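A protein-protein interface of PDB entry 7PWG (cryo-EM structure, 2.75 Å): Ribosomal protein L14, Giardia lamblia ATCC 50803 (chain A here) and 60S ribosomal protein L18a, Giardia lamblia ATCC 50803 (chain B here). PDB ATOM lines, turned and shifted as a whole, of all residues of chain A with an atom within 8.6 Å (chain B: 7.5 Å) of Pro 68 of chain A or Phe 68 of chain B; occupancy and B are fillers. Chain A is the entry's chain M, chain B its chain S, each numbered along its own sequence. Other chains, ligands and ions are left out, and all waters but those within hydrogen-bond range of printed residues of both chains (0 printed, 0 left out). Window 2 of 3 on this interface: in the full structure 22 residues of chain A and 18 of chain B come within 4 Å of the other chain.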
ATOM      1  N   ALA A   9      13.852  -1.432  -2.209  1.00  0.00           N
ATOM      2  CA  ALA A   9      13.823  -2.655  -1.425  1.00  0.00           C
ATOM      3  C   ALA A   9      14.204  -2.366   0.014  1.00  0.00           C
ATOM      4  O   ALA A   9      15.185  -1.672   0.285  1.00  0.00           O
ATOM      5  CB  ALA A   9      14.762  -3.690  -2.026  1.00  0.00           C
ATOM      6  N   GLY A  10      13.419  -2.906   0.940  1.00  0.00           N
ATOM      7  CA  GLY A  10      13.663  -2.729   2.350  1.00  0.00           C
ATOM      8  C   GLY A  10      13.062  -1.489   2.962  1.00  0.00           C
ATOM      9  O   GLY A  10      13.287  -1.237   4.148  1.00  0.00           O
ATOM     10  N   VAL A  26       6.914  -4.403   4.694  1.00  0.00           N
ATOM     11  CA  VAL A  26       8.159  -4.040   4.025  1.00  0.00           C
ATOM     12  C   VAL A  26       8.096  -4.431   2.557  1.00  0.00           C
ATOM     13  O   VAL A  26       7.472  -5.428   2.190  1.00  0.00           O
ATOM     14  CB  VAL A  26       9.390  -4.699   4.688  1.00  0.00           C
ATOM     15  CG1 VAL A  26      10.603  -3.803   4.547  1.00  0.00           C
ATOM     16  CG2 VAL A  26       9.122  -5.007   6.130  1.00  0.00           C
ATOM     17  N   ILE A  27       8.784  -3.664   1.719  1.00  0.00           N
ATOM     18  CA  ILE A  27       8.808  -3.874   0.274  1.00  0.00           C
ATOM     19  C   ILE A  27       9.905  -4.871  -0.088  1.00  0.00           C
ATOM     20  O   ILE A  27      11.033  -4.769   0.394  1.00  0.00           O
ATOM     21  CB  ILE A  27       9.015  -2.532  -0.456  1.00  0.00           C
ATOM     22  CG1 ILE A  27       7.788  -1.640  -0.314  1.00  0.00           C
ATOM     23  CG2 ILE A  27       9.309  -2.737  -1.915  1.00  0.00           C
ATOM     24  CD1 ILE A  27       8.081  -0.213  -0.490  1.00  0.00           C
ATOM     25  N   VAL A  28       9.585  -5.831  -0.961  1.00  0.00           N
ATOM     26  CA  VAL A  28      10.574  -6.800  -1.425  1.00  0.00           C
ATOM     27  C   VAL A  28      10.851  -6.648  -2.919  1.00  0.00           C
ATOM     28  O   VAL A  28      11.937  -7.004  -3.385  1.00  0.00           O
ATOM     29  CB  VAL A  28      10.151  -8.245  -1.088  1.00  0.00           C
ATOM     30  CG1 VAL A  28      10.063  -8.460   0.429  1.00  0.00           C
ATOM     31  CG2 VAL A  28       8.842  -8.585  -1.714  1.00  0.00           C
ATOM     32  N   ASP A  29       9.904  -6.109  -3.689  1.00  0.00           N
ATOM     33  CA  ASP A  29      10.144  -5.994  -5.121  1.00  0.00           C
ATOM     34  C   ASP A  29       9.265  -4.909  -5.738  1.00  0.00           C
ATOM     35  O   ASP A  29       8.257  -4.502  -5.167  1.00  0.00           O
ATOM     36  CB  ASP A  29       9.922  -7.332  -5.822  1.00  0.00           C
ATOM     37  CG  ASP A  29      11.011  -7.644  -6.817  1.00  0.00           C
ATOM     38  OD1 ASP A  29      11.849  -6.760  -7.069  1.00  0.00           O
ATOM     39  OD2 ASP A  29      11.043  -8.768  -7.348  1.00  0.00           O
ATOM     40  N   LEU A  31       7.288  -3.898  -9.080  1.00  0.00           N
ATOM     41  CA  LEU A  31       6.745  -4.259 -10.385  1.00  0.00           C
ATOM     42  C   LEU A  31       6.868  -3.104 -11.374  1.00  0.00           C
ATOM     43  O   LEU A  31       7.391  -3.274 -12.476  1.00  0.00           O
ATOM     44  CB  LEU A  31       5.293  -4.706 -10.247  1.00  0.00           C
ATOM     45  CG  LEU A  31       5.020  -6.131  -9.759  1.00  0.00           C
ATOM     46  CD1 LEU A  31       5.371  -6.331  -8.285  1.00  0.00           C
ATOM     47  CD2 LEU A  31       3.577  -6.473 -10.021  1.00  0.00           C
ATOM     48  N   LEU A  37       5.582  -5.462  -4.445  1.00  0.00           N
ATOM     49  CA  LEU A  37       5.387  -6.663  -3.647  1.00  0.00           C
ATOM     50  C   LEU A  37       5.778  -6.343  -2.211  1.00  0.00           C
ATOM     51  O   LEU A  37       6.909  -5.936  -1.952  1.00  0.00           O
ATOM     52  CB  LEU A  37       6.211  -7.824  -4.197  1.00  0.00           C
ATOM     53  CG  LEU A  37       5.963  -9.233  -3.658  1.00  0.00           C
ATOM     54  CD1 LEU A  37       4.540  -9.672  -3.881  1.00  0.00           C
ATOM     55  CD2 LEU A  37       6.916 -10.201  -4.309  1.00  0.00           C
ATOM     56  N   ASP A  39       5.555  -7.537   2.054  1.00  0.00           N
ATOM     57  CA  ASP A  39       5.400  -8.685   2.939  1.00  0.00           C
ATOM     58  C   ASP A  39       5.838  -8.273   4.335  1.00  0.00           C
ATOM     59  O   ASP A  39       7.035  -8.138   4.585  1.00  0.00           O
ATOM     60  CB  ASP A  39       6.219  -9.858   2.429  1.00  0.00           C
ATOM     61  CG  ASP A  39       6.039 -11.102   3.257  1.00  0.00           C
ATOM     62  OD1 ASP A  39       5.175 -11.130   4.154  1.00  0.00           O
ATOM     63  OD2 ASP A  39       6.772 -12.071   3.006  1.00  0.00           O
ATOM     64  N   ARG A  47       2.315 -11.957   2.048  1.00  0.00           N
ATOM     65  CA  ARG A  47       3.072 -11.411   0.925  1.00  0.00           C
ATOM     66  C   ARG A  47       2.164 -11.280  -0.289  1.00  0.00           C
ATOM     67  O   ARG A  47       1.696 -12.280  -0.834  1.00  0.00           O
ATOM     68  CB  ARG A  47       4.267 -12.299   0.604  1.00  0.00           C
ATOM     69  CG  ARG A  47       4.939 -11.922  -0.700  1.00  0.00           C
ATOM     70  CD  ARG A  47       6.190 -12.726  -0.947  1.00  0.00           C
ATOM     71  NE  ARG A  47       7.244 -12.382  -0.004  1.00  0.00           N
ATOM     72  CZ  ARG A  47       8.514 -12.735  -0.148  1.00  0.00           C
ATOM     73  NH1 ARG A  47       8.889 -13.441  -1.196  1.00  0.00           N
ATOM     74  NH2 ARG A  47       9.409 -12.377   0.760  1.00  0.00           N
ATOM     75  N   VAL A  49       0.617  -8.274  -3.591  1.00  0.00           N
ATOM     76  CA  VAL A  49       0.868  -7.107  -4.423  1.00  0.00           C
ATOM     77  C   VAL A  49      -0.135  -6.020  -4.073  1.00  0.00           C
ATOM     78  O   VAL A  49      -1.348  -6.256  -4.081  1.00  0.00           O
ATOM     79  CB  VAL A  49       0.798  -7.460  -5.916  1.00  0.00           C
ATOM     80  CG1 VAL A  49       0.702  -6.192  -6.748  1.00  0.00           C
ATOM     81  CG2 VAL A  49       2.023  -8.240  -6.317  1.00  0.00           C
ATOM     82  N   ASN A  63      17.741  -3.506   6.065  1.00  0.00           N
ATOM     83  CA  ASN A  63      18.713  -4.192   5.221  1.00  0.00           C
ATOM     84  C   ASN A  63      18.249  -5.624   4.993  1.00  0.00           C
ATOM     85  O   ASN A  63      18.052  -6.375   5.953  1.00  0.00           O
ATOM     86  CB  ASN A  63      20.102  -4.169   5.856  1.00  0.00           C
ATOM     87  CG  ASN A  63      21.193  -4.633   4.896  1.00  0.00           C
ATOM     88  OD1 ASN A  63      21.376  -5.830   4.675  1.00  0.00           O
ATOM     89  ND2 ASN A  63      21.919  -3.681   4.323  1.00  0.00           N
ATOM     90  N   ILE A  64      18.055  -5.995   3.725  1.00  0.00           N
ATOM     91  CA  ILE A  64      17.519  -7.297   3.351  1.00  0.00           C
ATOM     92  C   ILE A  64      18.287  -7.801   2.137  1.00  0.00           C
ATOM     93  O   ILE A  64      19.044  -7.063   1.504  1.00  0.00           O
ATOM     94  CB  ILE A  64      16.004  -7.250   3.041  1.00  0.00           C
ATOM     95  CG1 ILE A  64      15.721  -6.393   1.811  1.00  0.00           C
ATOM     96  CG2 ILE A  64      15.227  -6.710   4.208  1.00  0.00           C
ATOM     97  CD1 ILE A  64      14.295  -6.468   1.330  1.00  0.00           C
ATOM     98  N   SER A  65      18.076  -9.069   1.801  1.00  0.00           N
ATOM     99  CA  SER A  65      18.719  -9.636   0.622  1.00  0.00           C
ATOM    100  C   SER A  65      17.930  -9.234  -0.621  1.00  0.00           C
ATOM    101  O   SER A  65      17.011  -8.411  -0.572  1.00  0.00           O
ATOM    102  CB  SER A  65      18.834 -11.149   0.747  1.00  0.00           C
ATOM    103  OG  SER A  65      17.559 -11.743   0.663  1.00  0.00           O
ATOM    104  N   GLU A  66      18.269  -9.827  -1.760  1.00  0.00           N
ATOM    105  CA  GLU A  66      17.609  -9.441  -3.000  1.00  0.00           C
ATOM    106  C   GLU A  66      16.255 -10.128  -3.151  1.00  0.00           C
ATOM    107  O   GLU A  66      15.223  -9.461  -3.304  1.00  0.00           O
ATOM    108  CB  GLU A  66      18.530  -9.735  -4.179  1.00  0.00           C
ATOM    109  CG  GLU A  66      19.797  -8.922  -4.111  1.00  0.00           C
ATOM    110  CD  GLU A  66      20.705  -9.151  -5.284  1.00  0.00           C
ATOM    111  OE1 GLU A  66      21.919  -9.337  -5.062  1.00  0.00           O
ATOM    112  OE2 GLU A  66      20.207  -9.150  -6.428  1.00  0.00           O
ATOM    113  N   LYS A  67      16.229 -11.458  -3.087  1.00  0.00           N
ATOM    114  CA  LYS A  67      14.988 -12.228  -3.152  1.00  0.00           C
ATOM    115  C   LYS A  67      14.898 -13.073  -1.889  1.00  0.00           C
ATOM    116  O   LYS A  67      15.202 -14.277  -1.901  1.00  0.00           O
ATOM    117  CB  LYS A  67      14.928 -13.097  -4.404  1.00  0.00           C
ATOM    118  N   PRO A  68      14.491 -12.479  -0.776  1.00  0.00           N
ATOM    119  CA  PRO A  68      14.348 -13.256   0.454  1.00  0.00           C
ATOM    120  C   PRO A  68      13.108 -14.137   0.397  1.00  0.00           C
ATOM    121  O   PRO A  68      12.370 -14.178  -0.587  1.00  0.00           O
ATOM    122  CB  PRO A  68      14.246 -12.178   1.534  1.00  0.00           C
ATOM    123  CG  PRO A  68      13.674 -11.015   0.844  1.00  0.00           C
ATOM    124  CD  PRO A  68      14.145 -11.065  -0.584  1.00  0.00           C
ATOM    125  N   THR A  69      12.907 -14.878   1.476  1.00  0.00           N
ATOM    126  CA  THR A  69      11.761 -15.747   1.675  1.00  0.00           C
ATOM    127  C   THR A  69      11.089 -15.336   2.979  1.00  0.00           C
ATOM    128  O   THR A  69      11.715 -14.715   3.840  1.00  0.00           O
ATOM    129  CB  THR A  69      12.188 -17.226   1.725  1.00  0.00           C
ATOM    130  OG1 THR A  69      13.062 -17.521   0.631  1.00  0.00           O
ATOM    131  CG2 THR A  69      10.990 -18.150   1.656  1.00  0.00           C
ATOM    132  N   THR A  70       9.813 -15.691   3.140  1.00  0.00           N
ATOM    133  CA  THR A  70       9.070 -15.209   4.303  1.00  0.00           C
ATOM    134  C   THR A  70       9.714 -15.637   5.617  1.00  0.00           C
ATOM    135  O   THR A  70       9.448 -15.029   6.656  1.00  0.00           O
ATOM    136  CB  THR A  70       7.617 -15.677   4.259  1.00  0.00           C
ATOM    137  OG1 THR A  70       6.869 -14.994   5.270  1.00  0.00           O
ATOM    138  CG2 THR A  70       7.523 -17.147   4.526  1.00  0.00           C
ATOM    139  N   GLU A  71      10.552 -16.673   5.604  1.00  0.00           N
ATOM    140  CA  GLU A  71      11.295 -17.010   6.813  1.00  0.00           C
ATOM    141  C   GLU A  71      12.563 -16.177   6.935  1.00  0.00           C
ATOM    142  O   GLU A  71      12.872 -15.659   8.011  1.00  0.00           O
ATOM    143  CB  GLU A  71      11.645 -18.492   6.835  1.00  0.00           C
ATOM    144  CG  GLU A  71      10.487 -19.390   7.070  1.00  0.00           C
ATOM    145  CD  GLU A  71      10.112 -20.150   5.834  1.00  0.00           C
ATOM    146  OE1 GLU A  71       9.193 -19.701   5.124  1.00  0.00           O
ATOM    147  OE2 GLU A  71      10.743 -21.193   5.571  1.00  0.00           O
ATOM    148  N   GLN A  72      13.333 -16.071   5.850  1.00  0.00           N
ATOM    149  CA  GLN A  72      14.559 -15.282   5.907  1.00  0.00           C
ATOM    150  C   GLN A  72      14.261 -13.821   6.195  1.00  0.00           C
ATOM    151  O   GLN A  72      14.937 -13.189   7.014  1.00  0.00           O
ATOM    152  CB  GLN A  72      15.333 -15.398   4.606  1.00  0.00           C
ATOM    153  CG  GLN A  72      16.677 -14.735   4.684  1.00  0.00           C
ATOM    154  CD  GLN A  72      17.760 -15.650   4.222  1.00  0.00           C
ATOM    155  OE1 GLN A  72      17.520 -16.537   3.408  1.00  0.00           O
ATOM    156  NE2 GLN A  72      18.962 -15.454   4.734  1.00  0.00           N
ATOM    157  N   LEU A  73      13.247 -13.273   5.532  1.00  0.00           N
ATOM    158  CA  LEU A  73      12.830 -11.909   5.818  1.00  0.00           C
ATOM    159  C   LEU A  73      12.452 -11.762   7.282  1.00  0.00           C
ATOM    160  O   LEU A  73      12.771 -10.751   7.914  1.00  0.00           O
ATOM    161  CB  LEU A  73      11.667 -11.530   4.907  1.00  0.00           C
ATOM    162  CG  LEU A  73      11.176 -10.089   4.925  1.00  0.00           C
ATOM    163  CD1 LEU A  73      12.221  -9.161   4.357  1.00  0.00           C
ATOM    164  CD2 LEU A  73       9.894  -9.978   4.140  1.00  0.00           C
ATOM    165  N   LYS A  74      11.811 -12.788   7.847  1.00  0.00           N
ATOM    166  CA  LYS A  74      11.362 -12.732   9.231  1.00  0.00           C
ATOM    167  C   LYS A  74      12.532 -12.590  10.194  1.00  0.00           C
ATOM    168  O   LYS A  74      12.450 -11.843  11.173  1.00  0.00           O
ATOM    169  CB  LYS A  74      10.542 -13.977   9.559  1.00  0.00           C
ATOM    170  CG  LYS A  74       9.123 -13.687  10.015  1.00  0.00           C
ATOM    171  CD  LYS A  74       8.515 -14.873  10.736  1.00  0.00           C
ATOM    172  CE  LYS A  74       9.135 -15.053  12.104  1.00  0.00           C
ATOM    173  NZ  LYS A  74       8.603 -14.078  13.085  1.00  0.00           N
ATOM    174  N   LYS A  75      13.631 -13.299   9.940  1.00  0.00           N
ATOM    175  CA  LYS A  75      14.787 -13.159  10.814  1.00  0.00           C
ATOM    176  C   LYS A  75      15.639 -11.955  10.436  1.00  0.00           C
ATOM    177  O   LYS A  75      16.351 -11.418  11.289  1.00  0.00           O
ATOM    178  CB  LYS A  75      15.619 -14.445  10.805  1.00  0.00           C
ATOM    179  CG  LYS A  75      16.151 -14.844   9.444  1.00  0.00           C
ATOM    180  N   GLU A  76      15.586 -11.522   9.177  1.00  0.00           N
ATOM    181  CA  GLU A  76      16.229 -10.271   8.791  1.00  0.00           C
ATOM    182  C   GLU A  76      15.574  -9.084   9.476  1.00  0.00           C
ATOM    183  O   GLU A  76      16.264  -8.180   9.953  1.00  0.00           O
ATOM    184  CB  GLU A  76      16.173 -10.097   7.276  1.00  0.00           C
ATOM    185  CG  GLU A  76      17.382 -10.630   6.549  1.00  0.00           C
ATOM    186  CD  GLU A  76      17.113 -10.903   5.080  1.00  0.00           C
ATOM    187  OE1 GLU A  76      18.065 -11.278   4.361  1.00  0.00           O
ATOM    188  OE2 GLU A  76      15.952 -10.750   4.644  1.00  0.00           O
ATOM    189  N   ILE A  77      14.242  -9.070   9.524  1.00  0.00           N
ATOM    190  CA  ILE A  77      13.528  -7.991  10.196  1.00  0.00           C
ATOM    191  C   ILE A  77      13.904  -7.944  11.668  1.00  0.00           C
ATOM    192  O   ILE A  77      14.305  -6.899  12.193  1.00  0.00           O
ATOM    193  CB  ILE A  77      12.011  -8.167  10.015  1.00  0.00           C
ATOM    194  CG1 ILE A  77      11.581  -7.762   8.615  1.00  0.00           C
ATOM    195  CG2 ILE A  77      11.247  -7.357  11.039  1.00  0.00           C
ATOM    196  CD1 ILE A  77      10.176  -8.156   8.309  1.00  0.00           C
ATOM    197  N   ASN B  65       1.743 -20.506  -8.020  1.00  0.00           N
ATOM    198  CA  ASN B  65       2.423 -19.875  -6.903  1.00  0.00           C
ATOM    199  C   ASN B  65       2.942 -18.502  -7.304  1.00  0.00           C
ATOM    200  O   ASN B  65       3.504 -18.324  -8.386  1.00  0.00           O
ATOM    201  CB  ASN B  65       3.575 -20.764  -6.444  1.00  0.00           C
ATOM    202  CG  ASN B  65       4.527 -20.067  -5.502  1.00  0.00           C
ATOM    203  OD1 ASN B  65       5.413 -19.332  -5.924  1.00  0.00           O
ATOM    204  ND2 ASN B  65       4.371 -20.328  -4.218  1.00  0.00           N
ATOM    205  N   GLY B  66       2.759 -17.531  -6.419  1.00  0.00           N
ATOM    206  CA  GLY B  66       3.286 -16.205  -6.651  1.00  0.00           C
ATOM    207  C   GLY B  66       4.642 -15.977  -6.015  1.00  0.00           C
ATOM    208  O   GLY B  66       5.619 -16.653  -6.341  1.00  0.00           O
ATOM    209  N   ASP B  67       4.719 -14.980  -5.145  1.00  0.00           N
ATOM    210  CA  ASP B  67       5.831 -14.790  -4.220  1.00  0.00           C
ATOM    211  C   ASP B  67       7.122 -14.303  -4.870  1.00  0.00           C
ATOM    212  O   ASP B  67       8.039 -13.897  -4.151  1.00  0.00           O
ATOM    213  CB  ASP B  67       6.091 -16.082  -3.438  1.00  0.00           C
ATOM    214  CG  ASP B  67       4.867 -16.546  -2.677  1.00  0.00           C
ATOM    215  OD1 ASP B  67       4.349 -15.770  -1.841  1.00  0.00           O
ATOM    216  OD2 ASP B  67       4.403 -17.681  -2.924  1.00  0.00           O
ATOM    217  N   PHE B  68       7.203 -14.283  -6.201  1.00  0.00           N
ATOM    218  CA  PHE B  68       8.327 -13.647  -6.876  1.00  0.00           C
ATOM    219  C   PHE B  68       7.846 -13.033  -8.183  1.00  0.00           C
ATOM    220  O   PHE B  68       6.899 -13.519  -8.802  1.00  0.00           O
ATOM    221  CB  PHE B  68       9.489 -14.623  -7.138  1.00  0.00           C
ATOM    222  CG  PHE B  68      10.012 -15.296  -5.896  1.00  0.00           C
ATOM    223  CD1 PHE B  68      10.782 -14.599  -4.979  1.00  0.00           C
ATOM    224  CD2 PHE B  68       9.722 -16.626  -5.642  1.00  0.00           C
ATOM    225  CE1 PHE B  68      11.243 -15.222  -3.823  1.00  0.00           C
ATOM    226  CE2 PHE B  68      10.186 -17.247  -4.504  1.00  0.00           C
ATOM    227  CZ  PHE B  68      10.948 -16.541  -3.591  1.00  0.00           C
ATOM    228  N   VAL B  69       8.541 -11.979  -8.613  1.00  0.00           N
ATOM    229  CA  VAL B  69       8.108 -11.108  -9.704  1.00  0.00           C
ATOM    230  C   VAL B  69       8.910 -11.443 -10.950  1.00  0.00           C
ATOM    231  O   VAL B  69      10.138 -11.307 -10.965  1.00  0.00           O
ATOM    232  CB  VAL B  69       8.272  -9.628  -9.329  1.00  0.00           C
ATOM    233  CG1 VAL B  69       7.840  -8.715 -10.477  1.00  0.00           C
ATOM    234  CG2 VAL B  69       7.484  -9.322  -8.071  1.00  0.00           C
ATOM    235  N   LYS B  70       8.212 -11.834 -12.010  1.00  0.00           N
ATOM    236  CA  LYS B  70       8.811 -12.290 -13.255  1.00  0.00           C
ATOM    237  C   LYS B  70       8.313 -11.427 -14.404  1.00  0.00           C
ATOM    238  O   LYS B  70       7.405 -10.618 -14.239  1.00  0.00           O
ATOM    239  CB  LYS B  70       8.475 -13.770 -13.488  1.00  0.00           C
ATOM    240  CG  LYS B  70       7.845 -14.410 -12.257  1.00  0.00           C
ATOM    241  CD  LYS B  70       7.748 -15.910 -12.334  1.00  0.00           C
ATOM    242  CE  LYS B  70       6.496 -16.337 -13.061  1.00  0.00           C
ATOM    243  NZ  LYS B  70       6.142 -17.767 -12.827  1.00  0.00           N
ATOM    244  N   ASN B  71       8.931 -11.589 -15.574  1.00  0.00           N
ATOM    245  CA  ASN B  71       8.506 -10.918 -16.795  1.00  0.00           C
ATOM    246  C   ASN B  71       7.700 -11.872 -17.664  1.00  0.00           C
ATOM    247  O   ASN B  71       7.954 -13.074 -17.690  1.00  0.00           O
ATOM    248  CB  ASN B  71       9.693 -10.410 -17.620  1.00  0.00           C
ATOM    249  CG  ASN B  71      10.726  -9.691 -16.797  1.00  0.00           C
ATOM    250  OD1 ASN B  71      10.562  -8.529 -16.462  1.00  0.00           O
ATOM    251  ND2 ASN B  71      11.818 -10.372 -16.497  1.00  0.00           N
ATOM    252  N   PHE B  72       6.743 -11.324 -18.406  1.00  0.00           N
ATOM    253  CA  PHE B  72       5.952 -12.111 -19.341  1.00  0.00           C
ATOM    254  C   PHE B  72       5.876 -11.403 -20.680  1.00  0.00           C
ATOM    255  O   PHE B  72       5.880 -10.177 -20.743  1.00  0.00           O
ATOM    256  CB  PHE B  72       4.551 -12.374 -18.806  1.00  0.00           C
ATOM    257  CG  PHE B  72       4.528 -13.264 -17.610  1.00  0.00           C
ATOM    258  CD1 PHE B  72       4.465 -14.631 -17.753  1.00  0.00           C
ATOM    259  CD2 PHE B  72       4.607 -12.732 -16.347  1.00  0.00           C
ATOM    260  CE1 PHE B  72       4.469 -15.445 -16.656  1.00  0.00           C
ATOM    261  CE2 PHE B  72       4.600 -13.531 -15.257  1.00  0.00           C
ATOM    262  CZ  PHE B  72       4.529 -14.896 -15.408  1.00  0.00           C
ATOM    263  N   ARG B  92       5.352  -6.969 -16.050  1.00  0.00           N
ATOM    264  CA  ARG B  92       5.917  -7.610 -14.873  1.00  0.00           C
ATOM    265  C   ARG B  92       4.792  -7.926 -13.905  1.00  0.00           C
ATOM    266  O   ARG B  92       4.070  -7.021 -13.480  1.00  0.00           O
ATOM    267  CB  ARG B  92       6.962  -6.727 -14.199  1.00  0.00           C
ATOM    268  CG  ARG B  92       8.306  -6.778 -14.852  1.00  0.00           C
ATOM    269  CD  ARG B  92       9.302  -5.896 -14.136  1.00  0.00           C
ATOM    270  NE  ARG B  92      10.267  -6.658 -13.355  1.00  0.00           N
ATOM    271  CZ  ARG B  92      10.396  -6.563 -12.040  1.00  0.00           C
ATOM    272  NH1 ARG B  92       9.628  -5.730 -11.362  1.00  0.00           N
ATOM    273  NH2 ARG B  92      11.303  -7.283 -11.409  1.00  0.00           N
ATOM    274  N   GLU B  93       4.660  -9.198 -13.538  1.00  0.00           N
ATOM    275  CA  GLU B  93       3.644  -9.625 -12.589  1.00  0.00           C
ATOM    276  C   GLU B  93       4.133 -10.875 -11.876  1.00  0.00           C
ATOM    277  O   GLU B  93       5.253 -11.338 -12.085  1.00  0.00           O
ATOM    278  CB  GLU B  93       2.292  -9.885 -13.268  1.00  0.00           C
ATOM    279  CG  GLU B  93       1.354  -8.698 -13.325  1.00  0.00           C
ATOM    280  CD  GLU B  93       0.757  -8.309 -11.974  1.00  0.00           C
ATOM    281  OE1 GLU B  93       0.875  -9.080 -11.007  1.00  0.00           O
ATOM    282  OE2 GLU B  93       0.155  -7.219 -11.883  1.00  0.00           O
ATOM    283  N   THR B  94       3.271 -11.431 -11.033  1.00  0.00           N
ATOM    284  CA  THR B  94       3.675 -12.523 -10.159  1.00  0.00           C
ATOM    285  C   THR B  94       3.184 -13.886 -10.633  1.00  0.00           C
ATOM    286  O   THR B  94       3.835 -14.894 -10.357  1.00  0.00           O
ATOM    287  CB  THR B  94       3.191 -12.247  -8.732  1.00  0.00           C
ATOM    288  OG1 THR B  94       3.575 -10.926  -8.341  1.00  0.00           O
ATOM    289  CG2 THR B  94       3.844 -13.140  -7.805  1.00  0.00           C
ATOM    290  N   THR B  95       2.070 -13.932 -11.361  1.00  0.00           N
ATOM    291  CA  THR B  95       1.552 -15.147 -11.972  1.00  0.00           C
ATOM    292  C   THR B  95       1.049 -14.807 -13.366  1.00  0.00           C
ATOM    293  O   THR B  95       0.794 -13.647 -13.679  1.00  0.00           O
ATOM    294  CB  THR B  95       0.423 -15.782 -11.141  1.00  0.00           C
ATOM    295  OG1 THR B  95      -0.660 -14.861 -10.985  1.00  0.00           O
ATOM    296  CG2 THR B  95       0.912 -16.183  -9.783  1.00  0.00           C
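NH1 of Arg 47 of chain A lies within hydrogen-bond range of O of Asp 67 of chain B (3.1 Å).
The backbone carbonyl oxygen (O) of Asp 29 of chain A is in hydrogen-bond range of the backbone NH (N) of Leu 37 of chain A, at 2.9 Å.
The side-chain amide nitrogen (ND2) of Asn 65 of chain B lies within hydrogen-bond range of the side-chain carboxylate (OD2) of Asp 67 of chain B (2.9 Å).
The backbone NH (N) of Val 28 of chain A is in hydrogen-bond range of the backbone carbonyl oxygen (O) of Leu 37 of chain A (2.9 Å).
The guanidinium group of Arg 47 of chain A lies within salt-bridge range of the side-chain carboxylate of Asp 39 of chain A, at 3.1 Å.
O of Glu 93 of chain B sits at hydrogen-bond distance from N of Lys 70 of chain B (3.0 Å).
Among the printed residues, merely in contact across the chains: Asp 29 of chain A with Val 69 of chain B (3.5 Å), Leu 31 of chain A with Val 69 of chain B (3.7 Å), Leu 31 of chain A with Arg 92 of chain B (3.4 Å), Leu 31 of chain A with Glu 93 of chain B (3.9 Å), Leu 37 of chain A with Asp 67 of chain B (3.9 Å), Leu 37 of chain A with Val 69 of chain B (3.9 Å), Arg 47 of chain A with Phe 68 of chain B (3.95 Å), Val 49 of chain A with Thr 94 of chain B (3.7 Å) and Pro 68 of chain A with Phe 68 of chain B (3.6 Å).
Of the printed residues of chain B, Asp 29 of chain A touches Val 69.
Of the printed residues of chain B, Leu 31 of chain A touches Val 69 (3.7 Å), Arg 92 (3.4 Å) and Glu 93 (3.9 Å).
Ile 64 of chain A touches none of the printed residues of chain B.
Of chain A, only Arg 47 and Pro 68 come within 4 Å of Phe 68 of chain B.
Of the printed residues of chain A, Thr 94 of chain B touches Val 49 (3.7 Å).
Along chain A the printed residues that touch a printed residue of chain B span positions 29 to 68.
Among the printed residues, 10 pairs touch across the chains.
Among the printed residues, no Asp or Glu carboxylate lies within 4 Å of a Lys or Arg side-chain nitrogen of the other chain.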
